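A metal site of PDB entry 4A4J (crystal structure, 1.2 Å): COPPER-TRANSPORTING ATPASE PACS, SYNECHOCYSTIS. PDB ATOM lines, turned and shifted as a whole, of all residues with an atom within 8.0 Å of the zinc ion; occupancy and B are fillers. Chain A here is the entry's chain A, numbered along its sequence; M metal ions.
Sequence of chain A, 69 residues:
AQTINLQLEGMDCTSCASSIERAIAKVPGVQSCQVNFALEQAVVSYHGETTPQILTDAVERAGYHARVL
The backbone NH of Ser 15 lies close to the side-chain sulfur of Cys 13. OH of Tyr 64 lies close to SG of Cys 16 (3.2 Å).
The zinc ion is bound by the side-chain carboxylate (OD1) of Asp 12 (1.9 Å), the side-chain sulfur (SG) of Cys 13 (2.3 Å) and the side-chain sulfur (SG) of Cys 16 (2.3 Å). The zinc ion has three donor atoms within binding distance.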
ATOM      1  N   GLY A  10     -20.909 -31.126  12.326  1.00  0.00           N
ATOM      2  CA  GLY A  10     -22.308 -31.104  12.723  1.00  0.00           C
ATOM      3  C   GLY A  10     -22.575 -30.333  14.018  1.00  0.00           C
ATOM      4  O   GLY A  10     -23.706 -30.248  14.497  1.00  0.00           O
ATOM      5  N   MET A  11     -21.535 -29.769  14.612  1.00  0.00           N
ATOM      6  CA  MET A  11     -21.710 -29.058  15.882  1.00  0.00           C
ATOM      7  C   MET A  11     -22.047 -27.606  15.584  1.00  0.00           C
ATOM      8  O   MET A  11     -21.195 -26.723  15.630  1.00  0.00           O
ATOM      9  CB  MET A  11     -20.450 -29.179  16.711  1.00  0.00           C
ATOM     10  CG  MET A  11     -20.617 -28.560  18.089  1.00  0.00           C
ATOM     11  SD  MET A  11     -19.159 -28.719  19.109  1.00  0.00           S
ATOM     12  CE  MET A  11     -17.911 -28.011  18.105  1.00  0.00           C
ATOM     13  N   ASP A  12     -23.303 -27.373  15.241  1.00  0.00           N
ATOM     14  CA  ASP A  12     -23.716 -26.048  14.790  1.00  0.00           C
ATOM     15  C   ASP A  12     -24.064 -25.069  15.921  1.00  0.00           C
ATOM     16  O   ASP A  12     -24.187 -23.865  15.684  1.00  0.00           O
ATOM     17  CB  ASP A  12     -24.959 -26.199  13.920  1.00  0.00           C
ATOM     18  CG  ASP A  12     -26.181 -26.531  14.742  1.00  0.00           C
ATOM     19  OD1 ASP A  12     -26.158 -27.610  15.369  1.00  0.00           O
ATOM     20  OD2 ASP A  12     -27.097 -25.692  14.830  1.00  0.00           O
ATOM     21  N   CYS A  13     -24.259 -25.586  17.127  1.00  0.00           N
ATOM     22  CA  CYS A  13     -24.774 -24.823  18.258  1.00  0.00           C
ATOM     23  C   CYS A  13     -24.211 -25.365  19.567  1.00  0.00           C
ATOM     24  O   CYS A  13     -23.651 -26.467  19.596  1.00  0.00           O
ATOM     25  CB  CYS A  13     -26.313 -24.850  18.265  1.00  0.00           C
ATOM     26  SG  CYS A  13     -27.037 -26.458  18.733  1.00  0.00           S
ATOM     27  N   THR A  14     -24.407 -24.632  20.656  1.00  0.00           N
ATOM     28  CA  THR A  14     -23.830 -25.039  21.918  1.00  0.00           C
ATOM     29  C   THR A  14     -24.598 -26.224  22.547  1.00  0.00           C
ATOM     30  O   THR A  14     -24.008 -26.979  23.305  1.00  0.00           O
ATOM     31  CB  THR A  14     -23.711 -23.873  22.905  1.00  0.00           C
ATOM     32  OG1 THR A  14     -24.981 -23.233  23.043  1.00  0.00           O
ATOM     33  CG2 THR A  14     -22.716 -22.842  22.428  1.00  0.00           C
ATOM     34  N   SER A  15     -25.870 -26.396  22.204  1.00  0.00           N
ATOM     35  CA  SER A  15     -26.600 -27.604  22.604  1.00  0.00           C
ATOM     36  C   SER A  15     -25.928 -28.836  22.014  1.00  0.00           C
ATOM     37  O   SER A  15     -25.737 -29.848  22.695  1.00  0.00           O
ATOM     38  CB  SER A  15     -28.068 -27.530  22.141  1.00  0.00           C
ATOM     39  OG  SER A  15     -28.764 -28.777  22.188  1.00  0.00           O
ATOM     40  N   CYS A  16     -25.602 -28.782  20.745  1.00  0.00           N
ATOM     41  CA  CYS A  16     -24.925 -29.887  20.096  1.00  0.00           C
ATOM     42  C   CYS A  16     -23.503 -30.083  20.647  1.00  0.00           C
ATOM     43  O   CYS A  16     -23.064 -31.219  20.788  1.00  0.00           O
ATOM     44  CB  CYS A  16     -24.920 -29.684  18.598  1.00  0.00           C
ATOM     45  SG  CYS A  16     -26.552 -29.964  17.837  1.00  0.00           S
ATOM     46  N   ALA A  17     -22.819 -28.993  21.015  1.00  0.00           N
ATOM     47  CA  ALA A  17     -21.536 -29.124  21.671  1.00  0.00           C
ATOM     48  C   ALA A  17     -21.691 -29.977  22.952  1.00  0.00           C
ATOM     49  O   ALA A  17     -20.867 -30.874  23.234  1.00  0.00           O
ATOM     50  CB  ALA A  17     -20.918 -27.776  21.963  1.00  0.00           C
ATOM     51  N   SER A  19     -24.140 -32.076  23.637  1.00  0.00           N
ATOM     52  CA  SER A  19     -24.458 -33.442  23.211  1.00  0.00           C
ATOM     53  C   SER A  19     -23.227 -34.280  22.925  1.00  0.00           C
ATOM     54  O   SER A  19     -23.157 -35.453  23.278  1.00  0.00           O
ATOM     55  CB  SER A  19     -25.402 -33.441  21.999  1.00  0.00           C
ATOM     56  OG  SER A  19     -26.672 -32.888  22.336  1.00  0.00           O
ATOM     57  N   PHE A  37     -16.192 -25.129  21.057  1.00  0.00           N
ATOM     58  CA  PHE A  37     -17.238 -24.822  20.099  1.00  0.00           C
ATOM     59  C   PHE A  37     -16.703 -23.985  18.929  1.00  0.00           C
ATOM     60  O   PHE A  37     -16.929 -24.321  17.760  1.00  0.00           O
ATOM     61  CB  PHE A  37     -18.386 -24.110  20.829  1.00  0.00           C
ATOM     62  CG  PHE A  37     -19.466 -23.641  19.921  1.00  0.00           C
ATOM     63  CD1 PHE A  37     -20.238 -24.526  19.208  1.00  0.00           C
ATOM     64  CD2 PHE A  37     -19.710 -22.284  19.797  1.00  0.00           C
ATOM     65  CE1 PHE A  37     -21.199 -24.082  18.350  1.00  0.00           C
ATOM     66  CE2 PHE A  37     -20.708 -21.827  18.958  1.00  0.00           C
ATOM     67  CZ  PHE A  37     -21.449 -22.732  18.237  1.00  0.00           C
ATOM     68  N   TYR A  64     -23.357 -37.165  15.027  1.00  0.00           N
ATOM     69  CA  TYR A  64     -22.419 -36.202  14.484  1.00  0.00           C
ATOM     70  C   TYR A  64     -21.315 -36.976  13.745  1.00  0.00           C
ATOM     71  O   TYR A  64     -21.483 -38.144  13.456  1.00  0.00           O
ATOM     72  CB  TYR A  64     -21.856 -35.294  15.612  1.00  0.00           C
ATOM     73  CG  TYR A  64     -22.941 -34.650  16.428  1.00  0.00           C
ATOM     74  CD1 TYR A  64     -23.537 -33.457  16.017  1.00  0.00           C
ATOM     75  CD2 TYR A  64     -23.443 -35.262  17.557  1.00  0.00           C
ATOM     76  CE1 TYR A  64     -24.575 -32.892  16.736  1.00  0.00           C
ATOM     77  CE2 TYR A  64     -24.477 -34.729  18.274  1.00  0.00           C
ATOM     78  CZ  TYR A  64     -25.040 -33.524  17.870  1.00  0.00           C
ATOM     79  OH  TYR A  64     -26.074 -33.016  18.635  1.00  0.00           O
HETATM   80 ZN    ZN M   1     -27.224 -27.927  16.965  1.00  0.00          ZN
